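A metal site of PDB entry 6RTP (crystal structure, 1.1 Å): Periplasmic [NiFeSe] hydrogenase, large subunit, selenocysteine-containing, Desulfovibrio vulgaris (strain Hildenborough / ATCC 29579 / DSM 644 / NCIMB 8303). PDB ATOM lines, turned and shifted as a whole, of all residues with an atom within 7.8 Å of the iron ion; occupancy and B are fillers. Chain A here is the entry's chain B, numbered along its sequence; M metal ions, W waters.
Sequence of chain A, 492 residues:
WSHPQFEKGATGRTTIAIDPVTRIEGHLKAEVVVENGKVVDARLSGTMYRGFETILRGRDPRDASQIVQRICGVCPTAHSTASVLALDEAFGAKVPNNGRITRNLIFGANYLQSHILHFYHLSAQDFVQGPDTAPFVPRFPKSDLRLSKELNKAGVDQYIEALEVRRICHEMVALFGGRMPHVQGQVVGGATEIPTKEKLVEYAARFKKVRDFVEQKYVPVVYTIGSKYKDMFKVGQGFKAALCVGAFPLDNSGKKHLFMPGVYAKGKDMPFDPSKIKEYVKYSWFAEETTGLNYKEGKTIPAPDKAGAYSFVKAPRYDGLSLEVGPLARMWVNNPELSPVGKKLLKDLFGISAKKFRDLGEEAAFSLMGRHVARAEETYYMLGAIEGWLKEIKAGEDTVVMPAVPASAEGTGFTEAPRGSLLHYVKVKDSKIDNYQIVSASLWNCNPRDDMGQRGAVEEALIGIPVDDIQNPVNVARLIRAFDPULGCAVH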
ATOM      1  N   GLU A  53     -14.269   6.693  -3.017  1.00  0.00           N
ATOM      2  CA  GLU A  53     -13.897   8.107  -3.041  1.00  0.00           C
ATOM      3  C   GLU A  53     -13.966   8.704  -4.442  1.00  0.00           C
ATOM      4  O   GLU A  53     -14.156   9.924  -4.579  1.00  0.00           O
ATOM      5  CB  GLU A  53     -12.510   8.296  -2.414  1.00  0.00           C
ATOM      6  CG  GLU A  53     -12.513   7.994  -0.899  1.00  0.00           C
ATOM      7  CD  GLU A  53     -11.185   7.537  -0.337  1.00  0.00           C
ATOM      8  OE1 GLU A  53     -10.374   6.955  -1.089  1.00  0.00           O
ATOM      9  OE2 GLU A  53     -10.962   7.715   0.886  1.00  0.00           O
ATOM     10  N   GLU A 279      -1.794  10.390   4.899  1.00  0.00           N
ATOM     11  CA  GLU A 279      -1.876   9.062   4.332  1.00  0.00           C
ATOM     12  C   GLU A 279      -0.757   8.848   3.321  1.00  0.00           C
ATOM     13  O   GLU A 279      -0.679   9.534   2.295  1.00  0.00           O
ATOM     14  CB  GLU A 279      -3.235   8.783   3.704  1.00  0.00           C
ATOM     15  CG  GLU A 279      -4.373   8.776   4.702  1.00  0.00           C
ATOM     16  CD  GLU A 279      -5.675   8.330   4.078  1.00  0.00           C
ATOM     17  OE1 GLU A 279      -6.349   9.143   3.428  1.00  0.00           O
ATOM     18  OE2 GLU A 279      -5.989   7.139   4.236  1.00  0.00           O
ATOM     19  N   PHE A 286      -1.366   2.855  -5.089  1.00  0.00           N
ATOM     20  CA  PHE A 286      -1.831   4.176  -5.485  1.00  0.00           C
ATOM     21  C   PHE A 286      -0.669   4.967  -6.074  1.00  0.00           C
ATOM     22  O   PHE A 286       0.488   4.697  -5.770  1.00  0.00           O
ATOM     23  CB  PHE A 286      -2.469   4.937  -4.317  1.00  0.00           C
ATOM     24  CG  PHE A 286      -3.654   4.213  -3.772  1.00  0.00           C
ATOM     25  CD1 PHE A 286      -4.870   4.259  -4.420  1.00  0.00           C
ATOM     26  CD2 PHE A 286      -3.522   3.382  -2.662  1.00  0.00           C
ATOM     27  CE1 PHE A 286      -5.977   3.528  -3.966  1.00  0.00           C
ATOM     28  CE2 PHE A 286      -4.611   2.638  -2.202  1.00  0.00           C
ATOM     29  CZ  PHE A 286      -5.832   2.714  -2.859  1.00  0.00           C
ATOM     30  N   TYR A 295      -6.231  14.324   4.702  1.00  0.00           N
ATOM     31  CA  TYR A 295      -7.491  13.940   4.066  1.00  0.00           C
ATOM     32  C   TYR A 295      -8.216  15.133   3.426  1.00  0.00           C
ATOM     33  O   TYR A 295      -8.941  14.936   2.449  1.00  0.00           O
ATOM     34  CB  TYR A 295      -8.395  13.208   5.076  1.00  0.00           C
ATOM     35  CG  TYR A 295      -8.692  14.052   6.292  1.00  0.00           C
ATOM     36  CD1 TYR A 295      -9.707  14.978   6.274  1.00  0.00           C
ATOM     37  CD2 TYR A 295      -7.918  13.947   7.437  1.00  0.00           C
ATOM     38  CE1 TYR A 295      -9.958  15.794   7.337  1.00  0.00           C
ATOM     39  CE2 TYR A 295      -8.164  14.757   8.524  1.00  0.00           C
ATOM     40  CZ  TYR A 295      -9.173  15.685   8.474  1.00  0.00           C
ATOM     41  OH  TYR A 295      -9.392  16.482   9.568  1.00  0.00           O
ATOM     42  N   LYS A 299      -6.351  12.224  -2.218  1.00  0.00           N
ATOM     43  CA  LYS A 299      -6.489  11.778  -3.604  1.00  0.00           C
ATOM     44  C   LYS A 299      -6.445  10.262  -3.624  1.00  0.00           C
ATOM     45  O   LYS A 299      -5.706   9.636  -2.851  1.00  0.00           O
ATOM     46  CB  LYS A 299      -5.380  12.326  -4.478  1.00  0.00           C
ATOM     47  CG  LYS A 299      -5.437  13.821  -4.673  1.00  0.00           C
ATOM     48  CD  LYS A 299      -4.415  14.312  -5.670  1.00  0.00           C
ATOM     49  CE  LYS A 299      -4.767  15.724  -6.160  1.00  0.00           C
ATOM     50  NZ  LYS A 299      -3.681  16.321  -6.988  1.00  0.00           N
ATOM     51  N   THR A 300      -7.206   9.676  -4.548  1.00  0.00           N
ATOM     52  CA  THR A 300      -7.354   8.231  -4.639  1.00  0.00           C
ATOM     53  C   THR A 300      -7.189   7.851  -6.113  1.00  0.00           C
ATOM     54  O   THR A 300      -8.144   7.897  -6.890  1.00  0.00           O
ATOM     55  CB  THR A 300      -8.656   7.777  -4.031  1.00  0.00           C
ATOM     56  OG1 THR A 300      -8.670   8.253  -2.688  1.00  0.00           O
ATOM     57  CG2 THR A 300      -8.759   6.263  -4.033  1.00  0.00           C
ATOM     58  N   PHE A 312      -4.076  -2.478  -1.032  1.00  0.00           N
ATOM     59  CA  PHE A 312      -4.973  -1.388  -1.385  1.00  0.00           C
ATOM     60  C   PHE A 312      -5.320  -0.501  -0.199  1.00  0.00           C
ATOM     61  O   PHE A 312      -6.075   0.462  -0.368  1.00  0.00           O
ATOM     62  CB  PHE A 312      -6.247  -1.903  -2.048  1.00  0.00           C
ATOM     63  CG  PHE A 312      -6.045  -2.428  -3.444  1.00  0.00           C
ATOM     64  CD1 PHE A 312      -5.675  -1.578  -4.474  1.00  0.00           C
ATOM     65  CD2 PHE A 312      -6.271  -3.765  -3.746  1.00  0.00           C
ATOM     66  CE1 PHE A 312      -5.516  -2.059  -5.773  1.00  0.00           C
ATOM     67  CE2 PHE A 312      -6.104  -4.245  -5.034  1.00  0.00           C
ATOM     68  CZ  PHE A 312      -5.725  -3.381  -6.045  1.00  0.00           C
ATOM     69  N   LYS A 314      -4.251   2.405   2.249  1.00  0.00           N
ATOM     70  CA  LYS A 314      -3.261   3.459   2.432  1.00  0.00           C
ATOM     71  C   LYS A 314      -2.653   3.338   3.840  1.00  0.00           C
ATOM     72  O   LYS A 314      -3.127   2.572   4.672  1.00  0.00           O
ATOM     73  CB  LYS A 314      -3.892   4.835   2.247  1.00  0.00           C
ATOM     74  CG  LYS A 314      -4.486   5.146   0.850  1.00  0.00           C
ATOM     75  CD  LYS A 314      -5.078   6.552   0.809  1.00  0.00           C
ATOM     76  CE  LYS A 314      -5.605   6.929  -0.566  1.00  0.00           C
ATOM     77  NZ  LYS A 314      -6.475   8.136  -0.486  1.00  0.00           N
ATOM     78  N   LEU A 423     -13.377   8.982  10.061  1.00  0.00           N
ATOM     79  CA  LEU A 423     -13.740  10.316   9.624  1.00  0.00           C
ATOM     80  C   LEU A 423     -14.063  10.297   8.130  1.00  0.00           C
ATOM     81  O   LEU A 423     -13.493   9.515   7.358  1.00  0.00           O
ATOM     82  CB  LEU A 423     -12.673  11.370   9.944  1.00  0.00           C
ATOM     83  CG  LEU A 423     -11.381  11.233   9.158  1.00  0.00           C
ATOM     84  CD1 LEU A 423     -11.438  12.018   7.841  1.00  0.00           C
ATOM     85  CD2 LEU A 423     -10.162  11.688   9.956  1.00  0.00           C
ATOM     86  N   TYR A 436     -14.364  13.529  -1.756  1.00  0.00           N
ATOM     87  CA  TYR A 436     -14.874  12.828  -0.580  1.00  0.00           C
ATOM     88  C   TYR A 436     -13.753  11.892  -0.154  1.00  0.00           C
ATOM     89  O   TYR A 436     -13.298  11.075  -0.944  1.00  0.00           O
ATOM     90  CB  TYR A 436     -16.155  12.052  -0.917  1.00  0.00           C
ATOM     91  CG  TYR A 436     -17.007  11.741   0.295  1.00  0.00           C
ATOM     92  CD1 TYR A 436     -16.651  10.773   1.204  1.00  0.00           C
ATOM     93  CD2 TYR A 436     -18.193  12.436   0.517  1.00  0.00           C
ATOM     94  CE1 TYR A 436     -17.447  10.484   2.303  1.00  0.00           C
ATOM     95  CE2 TYR A 436     -18.986  12.167   1.610  1.00  0.00           C
ATOM     96  CZ  TYR A 436     -18.616  11.189   2.493  1.00  0.00           C
ATOM     97  OH  TYR A 436     -19.433  10.928   3.559  1.00  0.00           O
ATOM     98  N   GLN A 437     -13.277  12.055   1.080  1.00  0.00           N
ATOM     99  CA  GLN A 437     -12.169  11.242   1.563  1.00  0.00           C
ATOM    100  C   GLN A 437     -12.567  10.574   2.873  1.00  0.00           C
ATOM    101  O   GLN A 437     -13.141  11.211   3.771  1.00  0.00           O
ATOM    102  CB  GLN A 437     -10.896  12.089   1.722  1.00  0.00           C
ATOM    103  CG  GLN A 437     -10.275  12.459   0.363  1.00  0.00           C
ATOM    104  CD  GLN A 437      -9.663  11.264  -0.348  1.00  0.00           C
ATOM    105  OE1 GLN A 437      -9.015  10.438   0.270  1.00  0.00           O
ATOM    106  NE2 GLN A 437      -9.844  11.192  -1.658  1.00  0.00           N
ATOM    107  N   ILE A 438     -12.206   9.296   2.989  1.00  0.00           N
ATOM    108  CA  ILE A 438     -12.573   8.448   4.112  1.00  0.00           C
ATOM    109  C   ILE A 438     -11.302   7.904   4.743  1.00  0.00           C
ATOM    110  O   ILE A 438     -10.422   7.377   4.049  1.00  0.00           O
ATOM    111  CB  ILE A 438     -13.488   7.315   3.638  1.00  0.00           C
ATOM    112  CG1 ILE A 438     -14.812   7.907   3.154  1.00  0.00           C
ATOM    113  CG2 ILE A 438     -13.702   6.286   4.742  1.00  0.00           C
ATOM    114  CD1 ILE A 438     -15.500   7.089   2.161  1.00  0.00           C
ATOM    115  N   VAL A 439     -11.203   8.044   6.053  1.00  0.00           N
ATOM    116  CA  VAL A 439     -10.103   7.536   6.857  1.00  0.00           C
ATOM    117  C   VAL A 439     -10.778   6.706   7.940  1.00  0.00           C
ATOM    118  O   VAL A 439     -11.380   7.261   8.868  1.00  0.00           O
ATOM    119  CB  VAL A 439      -9.259   8.665   7.427  1.00  0.00           C
ATOM    120  CG1 VAL A 439      -8.129   8.156   8.290  1.00  0.00           C
ATOM    121  CG2 VAL A 439      -8.703   9.527   6.296  1.00  0.00           C
ATOM    122  N   SER A 440     -10.730   5.372   7.815  1.00  0.00           N
ATOM    123  CA  SER A 440     -11.583   4.452   8.582  1.00  0.00           C
ATOM    124  C   SER A 440     -10.775   3.674   9.631  1.00  0.00           C
ATOM    125  O   SER A 440      -9.544   3.725   9.685  1.00  0.00           O
ATOM    126  CB  SER A 440     -12.239   3.469   7.620  1.00  0.00           C
ATOM    127  OG  SER A 440     -11.192   2.756   6.983  1.00  0.00           O
ATOM    128  N   LEU A 443      -8.494   0.809   8.409  1.00  0.00           N
ATOM    129  CA  LEU A 443      -7.381   1.505   7.787  1.00  0.00           C
ATOM    130  C   LEU A 443      -6.264   1.763   8.806  1.00  0.00           C
ATOM    131  O   LEU A 443      -5.095   1.472   8.550  1.00  0.00           O
ATOM    132  CB  LEU A 443      -7.877   2.805   7.161  1.00  0.00           C
ATOM    133  CG  LEU A 443      -6.827   3.844   6.800  1.00  0.00           C
ATOM    134  CD1 LEU A 443      -6.033   3.413   5.603  1.00  0.00           C
ATOM    135  CD2 LEU A 443      -7.504   5.182   6.556  1.00  0.00           C
ATOM    136  N   CYS A 489     -13.974  -1.695   4.921  1.00  0.00           N
ATOM    137  CA  CYS A 489     -13.713  -0.388   5.499  1.00  0.00           C
ATOM    138  C   CYS A 489     -12.305   0.088   5.217  1.00  0.00           C
ATOM    139  O   CYS A 489     -12.083   1.264   4.934  1.00  0.00           O
ATOM    140  CB  CYS A 489     -13.895  -0.423   7.017  1.00  0.00           C
ATOM    141  SG  CYS A 489     -15.611  -0.333   7.511  1.00  0.00           S
ATOM    142  N   ALA A 490     -11.307  -0.793   5.357  1.00  0.00           N
ATOM    143  CA  ALA A 490      -9.923  -0.342   5.287  1.00  0.00           C
ATOM    144  C   ALA A 490      -9.599   0.228   3.911  1.00  0.00           C
ATOM    145  O   ALA A 490      -8.850   1.209   3.794  1.00  0.00           O
ATOM    146  CB  ALA A 490      -8.965  -1.485   5.602  1.00  0.00           C
ATOM    147  N   VAL A 491     -10.132  -0.384   2.851  1.00  0.00           N
ATOM    148  CA  VAL A 491      -9.805  -0.003   1.477  1.00  0.00           C
ATOM    149  C   VAL A 491     -10.832   0.935   0.885  1.00  0.00           C
ATOM    150  O   VAL A 491     -10.470   1.894   0.191  1.00  0.00           O
ATOM    151  CB  VAL A 491      -9.660  -1.259   0.587  1.00  0.00           C
ATOM    152  CG1 VAL A 491      -9.392  -0.833  -0.820  1.00  0.00           C
ATOM    153  CG2 VAL A 491      -8.567  -2.188   1.059  1.00  0.00           C
ATOM    154  N   HIS A 492     -12.124   0.633   1.072  1.00  0.00           N
ATOM    155  CA  HIS A 492     -13.204   1.385   0.453  1.00  0.00           C
ATOM    156  C   HIS A 492     -12.968   1.616  -1.039  1.00  0.00           C
ATOM    157  O   HIS A 492     -12.615   0.631  -1.744  1.00  0.00           O
ATOM    158  CB  HIS A 492     -13.579   2.678   1.234  1.00  0.00           C
ATOM    159  CG  HIS A 492     -12.424   3.485   1.764  1.00  0.00           C
ATOM    160  ND1 HIS A 492     -11.734   3.142   2.902  1.00  0.00           N
ATOM    161  CD2 HIS A 492     -11.855   4.637   1.319  1.00  0.00           C
ATOM    162  CE1 HIS A 492     -10.787   4.038   3.134  1.00  0.00           C
ATOM    163  NE2 HIS A 492     -10.833   4.956   2.180  1.00  0.00           N
ATOM    164  OXT HIS A 492     -13.198   2.731  -1.530  1.00  0.00           O
HETATM  165 FE    FE M   1      -9.544   6.639   2.132  1.00  0.00          FE
HETATM  166  O   HOH W   1      -8.018   5.697   3.283  1.00  0.00           O
HETATM  167  O   HOH W   2      -8.514   5.830   0.333  1.00  0.00           O
HETATM  168  O   HOH W   3      -8.361   8.413   1.948  1.00  0.00           O
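Three residues have an atom within 4 Å of the iron ion: Glu 53, Ile 438 and His 492.
A ring nitrogen (NE2) of His 492 is bound to the iron ion (2.1 Å). The iron ion is bound by water W1 (2.1 Å). The iron ion is bound by water W3 (2.1 Å). OE2 of Glu 53 binds the iron ion (2.2 Å). The iron ion is bound by water W2, 2.2 Å away. O of Ile 438 is bound to the iron ion (2.2 Å).
Water W3 lies within hydrogen-bond range of the side-chain carboxylate (OE1) of Glu 279 (2.6 Å), the side-chain amide oxygen (OE1) of Gln 437 (2.7 Å) and the side-chain amino group (NZ) of Lys 314 (3.1 Å). Water W2 lies within hydrogen-bond range of the side-chain carboxylate of Glu 53 (2.6 Å) and the side-chain amino group of Lys 314 (3.2 Å).
O of Cys 489 is in hydrogen-bond range of ND1 of His 492 (2.8 Å). The side-chain carboxylate of Glu 53 sits close to the side-chain amide oxygen of Gln 437. OE1 of Glu 53 lies within hydrogen-bond range of OG1 of Thr 300 (2.7 Å).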
